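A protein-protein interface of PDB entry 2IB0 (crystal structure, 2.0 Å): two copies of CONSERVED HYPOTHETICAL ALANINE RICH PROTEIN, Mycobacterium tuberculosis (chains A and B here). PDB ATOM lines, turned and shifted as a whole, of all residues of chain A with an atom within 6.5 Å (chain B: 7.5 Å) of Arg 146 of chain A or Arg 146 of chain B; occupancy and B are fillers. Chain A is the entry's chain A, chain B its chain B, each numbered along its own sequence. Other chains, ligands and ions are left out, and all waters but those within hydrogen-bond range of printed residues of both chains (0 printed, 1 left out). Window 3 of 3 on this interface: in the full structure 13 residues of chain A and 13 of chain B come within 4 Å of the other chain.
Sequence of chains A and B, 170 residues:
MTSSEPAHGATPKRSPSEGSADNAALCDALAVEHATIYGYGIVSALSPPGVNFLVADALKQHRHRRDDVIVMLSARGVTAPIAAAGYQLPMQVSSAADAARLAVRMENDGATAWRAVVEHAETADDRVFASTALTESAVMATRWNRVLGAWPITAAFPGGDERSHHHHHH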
ATOM      1  N   LEU A  54     -20.271 -35.478  -4.513  1.00  0.00           N
ATOM      2  CA  LEU A  54     -19.740 -34.153  -4.180  1.00  0.00           C
ATOM      3  C   LEU A  54     -18.986 -34.160  -2.840  1.00  0.00           C
ATOM      4  O   LEU A  54     -17.856 -33.653  -2.728  1.00  0.00           O
ATOM      5  CB  LEU A  54     -20.877 -33.119  -4.218  1.00  0.00           C
ATOM      6  CG  LEU A  54     -20.663 -31.590  -4.060  1.00  0.00           C
ATOM      7  CD1 LEU A  54     -19.565 -31.081  -4.979  1.00  0.00           C
ATOM      8  CD2 LEU A  54     -21.969 -30.727  -4.243  1.00  0.00           C
ATOM      9  N   VAL A 139     -14.499 -23.024  -6.754  1.00  0.00           N
ATOM     10  CA  VAL A 139     -15.255 -23.937  -7.608  1.00  0.00           C
ATOM     11  C   VAL A 139     -16.129 -24.832  -6.688  1.00  0.00           C
ATOM     12  O   VAL A 139     -17.340 -25.020  -6.942  1.00  0.00           O
ATOM     13  CB  VAL A 139     -14.307 -24.724  -8.514  1.00  0.00           C
ATOM     14  CG1 VAL A 139     -14.998 -25.936  -9.105  1.00  0.00           C
ATOM     15  CG2 VAL A 139     -13.725 -23.778  -9.654  1.00  0.00           C
ATOM     16  N   ALA A 141     -17.447 -24.120  -3.667  1.00  0.00           N
ATOM     17  CA  ALA A 141     -18.553 -23.240  -3.236  1.00  0.00           C
ATOM     18  C   ALA A 141     -19.608 -23.064  -4.330  1.00  0.00           C
ATOM     19  O   ALA A 141     -20.818 -23.108  -4.031  1.00  0.00           O
ATOM     20  CB  ALA A 141     -18.024 -21.836  -2.727  1.00  0.00           C
ATOM     21  N   THR A 142     -19.194 -22.849  -5.589  1.00  0.00           N
ATOM     22  CA  THR A 142     -20.192 -22.661  -6.624  1.00  0.00           C
ATOM     23  C   THR A 142     -20.984 -23.971  -6.827  1.00  0.00           C
ATOM     24  O   THR A 142     -22.172 -23.940  -7.113  1.00  0.00           O
ATOM     25  CB  THR A 142     -19.605 -22.223  -8.019  1.00  0.00           C
ATOM     26  OG1 THR A 142     -18.911 -23.330  -8.594  1.00  0.00           O
ATOM     27  CG2 THR A 142     -18.651 -21.085  -7.890  1.00  0.00           C
ATOM     28  N   ARG A 143     -20.308 -25.116  -6.748  1.00  0.00           N
ATOM     29  CA  ARG A 143     -20.992 -26.413  -6.849  1.00  0.00           C
ATOM     30  C   ARG A 143     -22.045 -26.654  -5.731  1.00  0.00           C
ATOM     31  O   ARG A 143     -23.105 -27.182  -5.990  1.00  0.00           O
ATOM     32  CB  ARG A 143     -19.965 -27.557  -6.843  1.00  0.00           C
ATOM     33  CG  ARG A 143     -19.106 -27.498  -8.050  1.00  0.00           C
ATOM     34  CD  ARG A 143     -18.016 -28.599  -8.144  1.00  0.00           C
ATOM     35  NE  ARG A 143     -18.641 -29.915  -8.299  1.00  0.00           N
ATOM     36  CZ  ARG A 143     -18.069 -31.096  -8.027  1.00  0.00           C
ATOM     37  NH1 ARG A 143     -16.808 -31.190  -7.560  1.00  0.00           N
ATOM     38  NH2 ARG A 143     -18.780 -32.213  -8.214  1.00  0.00           N
ATOM     39  N   TRP A 144     -21.752 -26.261  -4.507  1.00  0.00           N
ATOM     40  CA  TRP A 144     -22.725 -26.369  -3.413  1.00  0.00           C
ATOM     41  C   TRP A 144     -23.862 -25.350  -3.504  1.00  0.00           C
ATOM     42  O   TRP A 144     -24.981 -25.644  -3.111  1.00  0.00           O
ATOM     43  CB  TRP A 144     -22.031 -26.284  -2.047  1.00  0.00           C
ATOM     44  CG  TRP A 144     -21.332 -27.543  -1.688  1.00  0.00           C
ATOM     45  CD1 TRP A 144     -19.979 -27.793  -1.744  1.00  0.00           C
ATOM     46  CD2 TRP A 144     -21.952 -28.754  -1.195  1.00  0.00           C
ATOM     47  NE1 TRP A 144     -19.723 -29.099  -1.329  1.00  0.00           N
ATOM     48  CE2 TRP A 144     -20.913 -29.700  -0.973  1.00  0.00           C
ATOM     49  CE3 TRP A 144     -23.285 -29.122  -0.910  1.00  0.00           C
ATOM     50  CZ2 TRP A 144     -21.167 -31.018  -0.477  1.00  0.00           C
ATOM     51  CZ3 TRP A 144     -23.536 -30.442  -0.413  1.00  0.00           C
ATOM     52  CH2 TRP A 144     -22.471 -31.360  -0.215  1.00  0.00           C
ATOM     53  N   ASN A 145     -23.568 -24.161  -4.055  1.00  0.00           N
ATOM     54  CA  ASN A 145     -24.567 -23.153  -4.320  1.00  0.00           C
ATOM     55  C   ASN A 145     -25.542 -23.597  -5.418  1.00  0.00           C
ATOM     56  O   ASN A 145     -26.719 -23.253  -5.389  1.00  0.00           O
ATOM     57  CB  ASN A 145     -23.892 -21.862  -4.739  1.00  0.00           C
ATOM     58  CG  ASN A 145     -23.665 -20.911  -3.580  1.00  0.00           C
ATOM     59  OD1 ASN A 145     -22.551 -20.327  -3.423  1.00  0.00           O
ATOM     60  ND2 ASN A 145     -24.714 -20.705  -2.770  1.00  0.00           N
ATOM     61  N   ARG A 146     -25.023 -24.340  -6.388  1.00  0.00           N
ATOM     62  CA  ARG A 146     -25.824 -24.939  -7.426  1.00  0.00           C
ATOM     63  C   ARG A 146     -26.736 -26.027  -6.817  1.00  0.00           C
ATOM     64  O   ARG A 146     -27.892 -26.146  -7.206  1.00  0.00           O
ATOM     65  CB  ARG A 146     -24.916 -25.531  -8.501  1.00  0.00           C
ATOM     66  CG  ARG A 146     -25.599 -25.953  -9.756  1.00  0.00           C
ATOM     67  CD  ARG A 146     -24.519 -26.120 -10.858  1.00  0.00           C
ATOM     68  NE  ARG A 146     -23.977 -24.818 -11.290  1.00  0.00           N
ATOM     69  CZ  ARG A 146     -22.681 -24.539 -11.515  1.00  0.00           C
ATOM     70  NH1 ARG A 146     -21.731 -25.449 -11.345  1.00  0.00           N
ATOM     71  NH2 ARG A 146     -22.337 -23.317 -11.897  1.00  0.00           N
ATOM     72  N   VAL A 147     -26.219 -26.800  -5.858  1.00  0.00           N
ATOM     73  CA  VAL A 147     -27.071 -27.696  -5.079  1.00  0.00           C
ATOM     74  C   VAL A 147     -28.201 -26.939  -4.343  1.00  0.00           C
ATOM     75  O   VAL A 147     -29.387 -27.281  -4.487  1.00  0.00           O
ATOM     76  CB  VAL A 147     -26.213 -28.594  -4.114  1.00  0.00           C
ATOM     77  CG1 VAL A 147     -27.124 -29.439  -3.202  1.00  0.00           C
ATOM     78  CG2 VAL A 147     -25.309 -29.519  -4.942  1.00  0.00           C
ATOM     79  N   LEU A 148     -27.871 -25.912  -3.549  1.00  0.00           N
ATOM     80  CA  LEU A 148     -28.914 -25.114  -2.853  1.00  0.00           C
ATOM     81  C   LEU A 148     -29.968 -24.580  -3.806  1.00  0.00           C
ATOM     82  O   LEU A 148     -31.141 -24.665  -3.514  1.00  0.00           O
ATOM     83  CB  LEU A 148     -28.294 -23.917  -2.122  1.00  0.00           C
ATOM     84  CG  LEU A 148     -27.571 -24.283  -0.829  1.00  0.00           C
ATOM     85  CD1 LEU A 148     -26.817 -23.060  -0.276  1.00  0.00           C
ATOM     86  CD2 LEU A 148     -28.601 -24.810   0.177  1.00  0.00           C
ATOM     87  N   GLY A 149     -29.526 -23.958  -4.917  1.00  0.00           N
ATOM     88  CA  GLY A 149     -30.412 -23.357  -5.937  1.00  0.00           C
ATOM     89  C   GLY A 149     -31.390 -24.315  -6.603  1.00  0.00           C
ATOM     90  O   GLY A 149     -32.413 -23.891  -7.119  1.00  0.00           O
ATOM     91  N   ALA A 150     -31.046 -25.602  -6.643  1.00  0.00           N
ATOM     92  CA  ALA A 150     -31.925 -26.682  -7.090  1.00  0.00           C
ATOM     93  C   ALA A 150     -32.857 -27.234  -5.981  1.00  0.00           C
ATOM     94  O   ALA A 150     -33.752 -28.064  -6.261  1.00  0.00           O
ATOM     95  CB  ALA A 150     -31.071 -27.838  -7.680  1.00  0.00           C
ATOM     96  N   TRP A 151     -32.663 -26.807  -4.737  1.00  0.00           N
ATOM     97  CA  TRP A 151     -33.602 -27.199  -3.716  1.00  0.00           C
ATOM     98  C   TRP A 151     -34.603 -26.089  -3.443  1.00  0.00           C
ATOM     99  O   TRP A 151     -34.301 -24.932  -3.707  1.00  0.00           O
ATOM    100  CB  TRP A 151     -32.898 -27.558  -2.416  1.00  0.00           C
ATOM    101  CG  TRP A 151     -32.025 -28.750  -2.512  1.00  0.00           C
ATOM    102  CD1 TRP A 151     -32.067 -29.727  -3.450  1.00  0.00           C
ATOM    103  CD2 TRP A 151     -31.025 -29.136  -1.546  1.00  0.00           C
ATOM    104  NE1 TRP A 151     -31.104 -30.674  -3.172  1.00  0.00           N
ATOM    105  CE2 TRP A 151     -30.436 -30.327  -2.016  1.00  0.00           C
ATOM    106  CE3 TRP A 151     -30.547 -28.558  -0.360  1.00  0.00           C
ATOM    107  CZ2 TRP A 151     -29.424 -30.992  -1.317  1.00  0.00           C
ATOM    108  CZ3 TRP A 151     -29.491 -29.232   0.365  1.00  0.00           C
ATOM    109  CH2 TRP A 151     -28.955 -30.424  -0.136  1.00  0.00           C
ATOM    110  N   LEU B  54     -25.696 -15.841 -18.382  1.00  0.00           N
ATOM    111  CA  LEU B  54     -24.317 -16.362 -18.299  1.00  0.00           C
ATOM    112  C   LEU B  54     -23.381 -15.590 -19.223  1.00  0.00           C
ATOM    113  O   LEU B  54     -22.280 -15.224 -18.837  1.00  0.00           O
ATOM    114  CB  LEU B  54     -24.253 -17.857 -18.633  1.00  0.00           C
ATOM    115  CG  LEU B  54     -22.909 -18.581 -18.436  1.00  0.00           C
ATOM    116  CD1 LEU B  54     -22.249 -18.348 -17.044  1.00  0.00           C
ATOM    117  CD2 LEU B  54     -23.106 -20.071 -18.649  1.00  0.00           C
ATOM    118  N   ALA B 100     -20.554 -23.341 -26.238  1.00  0.00           N
ATOM    119  CA  ALA B 100     -20.206 -23.696 -24.857  1.00  0.00           C
ATOM    120  C   ALA B 100     -18.767 -24.176 -24.785  1.00  0.00           C
ATOM    121  O   ALA B 100     -18.042 -23.796 -23.874  1.00  0.00           O
ATOM    122  CB  ALA B 100     -21.170 -24.812 -24.311  1.00  0.00           C
ATOM    123  N   VAL B 104     -15.649 -22.606 -22.707  1.00  0.00           N
ATOM    124  CA  VAL B 104     -14.805 -23.419 -21.817  1.00  0.00           C
ATOM    125  C   VAL B 104     -13.313 -23.235 -22.163  1.00  0.00           C
ATOM    126  O   VAL B 104     -12.488 -23.006 -21.271  1.00  0.00           O
ATOM    127  CB  VAL B 104     -15.210 -24.927 -21.822  1.00  0.00           C
ATOM    128  CG1 VAL B 104     -14.177 -25.820 -21.054  1.00  0.00           C
ATOM    129  CG2 VAL B 104     -16.611 -25.096 -21.231  1.00  0.00           C
ATOM    130  N   VAL B 139     -14.076 -20.610 -12.467  1.00  0.00           N
ATOM    131  CA  VAL B 139     -15.488 -20.718 -12.143  1.00  0.00           C
ATOM    132  C   VAL B 139     -16.300 -20.576 -13.436  1.00  0.00           C
ATOM    133  O   VAL B 139     -17.260 -21.315 -13.669  1.00  0.00           O
ATOM    134  CB  VAL B 139     -15.929 -19.704 -11.101  1.00  0.00           C
ATOM    135  CG1 VAL B 139     -17.436 -19.584 -11.112  1.00  0.00           C
ATOM    136  CG2 VAL B 139     -15.445 -20.119  -9.656  1.00  0.00           C
ATOM    137  N   MET B 140     -15.901 -19.656 -14.302  1.00  0.00           N
ATOM    138  CA  MET B 140     -16.643 -19.450 -15.527  1.00  0.00           C
ATOM    139  C   MET B 140     -16.565 -20.726 -16.432  1.00  0.00           C
ATOM    140  O   MET B 140     -17.583 -21.187 -16.956  1.00  0.00           O
ATOM    141  CB  MET B 140     -16.134 -18.164 -16.200  1.00  0.00           C
ATOM    142  CG  MET B 140     -17.105 -17.492 -17.113  1.00  0.00           C
ATOM    143  SD  MET B 140     -18.830 -17.258 -16.633  1.00  0.00           S
ATOM    144  CE  MET B 140     -18.836 -15.839 -15.596  1.00  0.00           C
ATOM    145  N   ALA B 141     -15.376 -21.326 -16.570  1.00  0.00           N
ATOM    146  CA  ALA B 141     -15.248 -22.582 -17.296  1.00  0.00           C
ATOM    147  C   ALA B 141     -16.170 -23.685 -16.749  1.00  0.00           C
ATOM    148  O   ALA B 141     -16.829 -24.382 -17.519  1.00  0.00           O
ATOM    149  CB  ALA B 141     -13.831 -23.023 -17.315  1.00  0.00           C
ATOM    150  N   THR B 142     -16.262 -23.823 -15.428  1.00  0.00           N
ATOM    151  CA  THR B 142     -17.157 -24.824 -14.870  1.00  0.00           C
ATOM    152  C   THR B 142     -18.629 -24.547 -15.217  1.00  0.00           C
ATOM    153  O   THR B 142     -19.355 -25.454 -15.540  1.00  0.00           O
ATOM    154  CB  THR B 142     -16.979 -25.009 -13.346  1.00  0.00           C
ATOM    155  OG1 THR B 142     -17.337 -23.799 -12.690  1.00  0.00           O
ATOM    156  CG2 THR B 142     -15.542 -25.349 -13.015  1.00  0.00           C
ATOM    157  N   ARG B 143     -19.051 -23.293 -15.174  1.00  0.00           N
ATOM    158  CA  ARG B 143     -20.416 -22.917 -15.477  1.00  0.00           C
ATOM    159  C   ARG B 143     -20.780 -23.231 -16.937  1.00  0.00           C
ATOM    160  O   ARG B 143     -21.877 -23.706 -17.220  1.00  0.00           O
ATOM    161  CB  ARG B 143     -20.635 -21.443 -15.144  1.00  0.00           C
ATOM    162  CG  ARG B 143     -20.554 -21.139 -13.634  1.00  0.00           C
ATOM    163  CD  ARG B 143     -20.772 -19.662 -13.396  1.00  0.00           C
ATOM    164  NE  ARG B 143     -22.150 -19.282 -13.718  1.00  0.00           N
ATOM    165  CZ  ARG B 143     -22.594 -18.027 -13.851  1.00  0.00           C
ATOM    166  NH1 ARG B 143     -21.768 -16.991 -13.692  1.00  0.00           N
ATOM    167  NH2 ARG B 143     -23.876 -17.813 -14.141  1.00  0.00           N
ATOM    168  N   TRP B 144     -19.845 -23.026 -17.854  1.00  0.00           N
ATOM    169  CA  TRP B 144     -20.105 -23.331 -19.270  1.00  0.00           C
ATOM    170  C   TRP B 144     -19.952 -24.813 -19.507  1.00  0.00           C
ATOM    171  O   TRP B 144     -20.544 -25.369 -20.423  1.00  0.00           O
ATOM    172  CB  TRP B 144     -19.135 -22.586 -20.150  1.00  0.00           C
ATOM    173  CG  TRP B 144     -19.559 -21.211 -20.383  1.00  0.00           C
ATOM    174  CD1 TRP B 144     -19.041 -20.093 -19.802  1.00  0.00           C
ATOM    175  CD2 TRP B 144     -20.573 -20.767 -21.322  1.00  0.00           C
ATOM    176  NE1 TRP B 144     -19.674 -18.972 -20.299  1.00  0.00           N
ATOM    177  CE2 TRP B 144     -20.625 -19.353 -21.224  1.00  0.00           C
ATOM    178  CE3 TRP B 144     -21.473 -21.436 -22.188  1.00  0.00           C
ATOM    179  CZ2 TRP B 144     -21.523 -18.568 -21.978  1.00  0.00           C
ATOM    180  CZ3 TRP B 144     -22.386 -20.642 -22.972  1.00  0.00           C
ATOM    181  CH2 TRP B 144     -22.395 -19.227 -22.848  1.00  0.00           C
ATOM    182  N   ASN B 145     -19.168 -25.462 -18.658  1.00  0.00           N
ATOM    183  CA  ASN B 145     -19.054 -26.904 -18.760  1.00  0.00           C
ATOM    184  C   ASN B 145     -20.320 -27.663 -18.337  1.00  0.00           C
ATOM    185  O   ASN B 145     -20.592 -28.780 -18.807  1.00  0.00           O
ATOM    186  CB  ASN B 145     -17.848 -27.397 -18.014  1.00  0.00           C
ATOM    187  CG  ASN B 145     -17.331 -28.659 -18.588  1.00  0.00           C
ATOM    188  OD1 ASN B 145     -17.449 -29.727 -17.965  1.00  0.00           O
ATOM    189  ND2 ASN B 145     -16.784 -28.580 -19.789  1.00  0.00           N
ATOM    190  N   ARG B 146     -21.096 -27.041 -17.457  1.00  0.00           N
ATOM    191  CA  ARG B 146     -22.427 -27.521 -17.132  1.00  0.00           C
ATOM    192  C   ARG B 146     -23.482 -27.216 -18.217  1.00  0.00           C
ATOM    193  O   ARG B 146     -24.529 -27.883 -18.268  1.00  0.00           O
ATOM    194  CB  ARG B 146     -22.820 -27.058 -15.721  1.00  0.00           C
ATOM    195  CG  ARG B 146     -21.871 -27.670 -14.653  1.00  0.00           C
ATOM    196  CD  ARG B 146     -22.574 -28.072 -13.356  1.00  0.00           C
ATOM    197  NE  ARG B 146     -22.142 -29.362 -12.762  1.00  0.00           N
ATOM    198  CZ  ARG B 146     -21.593 -29.538 -11.544  1.00  0.00           C
ATOM    199  NH1 ARG B 146     -21.343 -28.506 -10.749  1.00  0.00           N
ATOM    200  NH2 ARG B 146     -21.282 -30.761 -11.130  1.00  0.00           N
ATOM    201  N   VAL B 147     -23.196 -26.247 -19.097  1.00  0.00           N
ATOM    202  CA  VAL B 147     -24.015 -25.995 -20.316  1.00  0.00           C
ATOM    203  C   VAL B 147     -23.880 -27.162 -21.331  1.00  0.00           C
ATOM    204  O   VAL B 147     -24.891 -27.741 -21.783  1.00  0.00           O
ATOM    205  CB  VAL B 147     -23.720 -24.600 -20.944  1.00  0.00           C
ATOM    206  CG1 VAL B 147     -24.452 -24.366 -22.346  1.00  0.00           C
ATOM    207  CG2 VAL B 147     -24.093 -23.498 -19.969  1.00  0.00           C
ATOM    208  N   LEU B 148     -22.651 -27.573 -21.641  1.00  0.00           N
ATOM    209  CA  LEU B 148     -22.480 -28.829 -22.408  1.00  0.00           C
ATOM    210  C   LEU B 148     -22.431 -30.110 -21.571  1.00  0.00           C
ATOM    211  O   LEU B 148     -23.122 -30.266 -20.544  1.00  0.00           O
ATOM    212  CB  LEU B 148     -21.261 -28.724 -23.353  1.00  0.00           C
ATOM    213  CG  LEU B 148     -19.876 -28.671 -22.735  1.00  0.00           C
ATOM    214  CD1 LEU B 148     -18.788 -28.885 -23.736  1.00  0.00           C
ATOM    215  CD2 LEU B 148     -19.711 -27.338 -22.160  1.00  0.00           C
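NH1 of Arg 146 of chain A sits close to NH1 of Arg 146 of chain B (3.1 Å).
The backbone carbonyl oxygen (O) of Val 139 of chain B sits at hydrogen-bond distance from the side-chain hydroxyl (OG1) of Thr 142 of chain B, at 2.7 Å. O of Val 139 of chain A sits at hydrogen-bond distance from OG1 of Thr 142 of chain A, 2.8 Å away.
Val 139 of chain A touches Thr 142 of chain B (CG1 to CG2, 3.99 Å). Val 139 of chain B touches Thr 142 of chain A (CG1 to CG2, 3.8 Å). Arg 143 of chain A touches Arg 146 of chain B. CG of Arg 143 of chain B touches NH2 of Arg 146 of chain A, 3.3 Å away.
Arg 146 of chain A touches just these residues of chain B: Arg 143 and Arg 146. Printed residues of chain A within 4 Å of Thr 142 of chain B: Val 139. Printed residues of chain A within 4 Å of Arg 143 of chain B: Arg 146 (3.3 Å). Of chain A, only Arg 143 and Arg 146 come within 4 Å of Arg 146 of chain B.
Of the 13 printed residues of chain B, 4 touch a printed residue of chain A. Printed residues of chain B that touch a printed residue of chain A: Val 139, Thr 142, Arg 143 and Arg 146. Of the 13 printed residues of chain A, 4 touch a printed residue of chain B. Hydrophobic or aromatic side chains of chain A that line the printed part of chain B: Val 139. Among the printed residues, no Asp or Glu carboxylate lies within 4 Å of a Lys or Arg side-chain nitrogen of the other chain.
Val 139 of chain A touches Thr 142 of chain B, and with the chains exchanged Thr 142 of chain A touches Val 139 of chain B. Arg 143 of chain A touches Arg 146 of chain B, and with the chains exchanged Arg 146 of chain A touches Arg 143 of chain B. Arg 146 of chain A touches its own counterpart, Arg 146 of chain B. Positions printed for both chains: 54, 139, 141, 142, 143, 144, 145, 146, 147 and 148. Of the 5 pairs that touch across the chains among the printed residues, 5 have their exchanged pair printed and touching as well.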
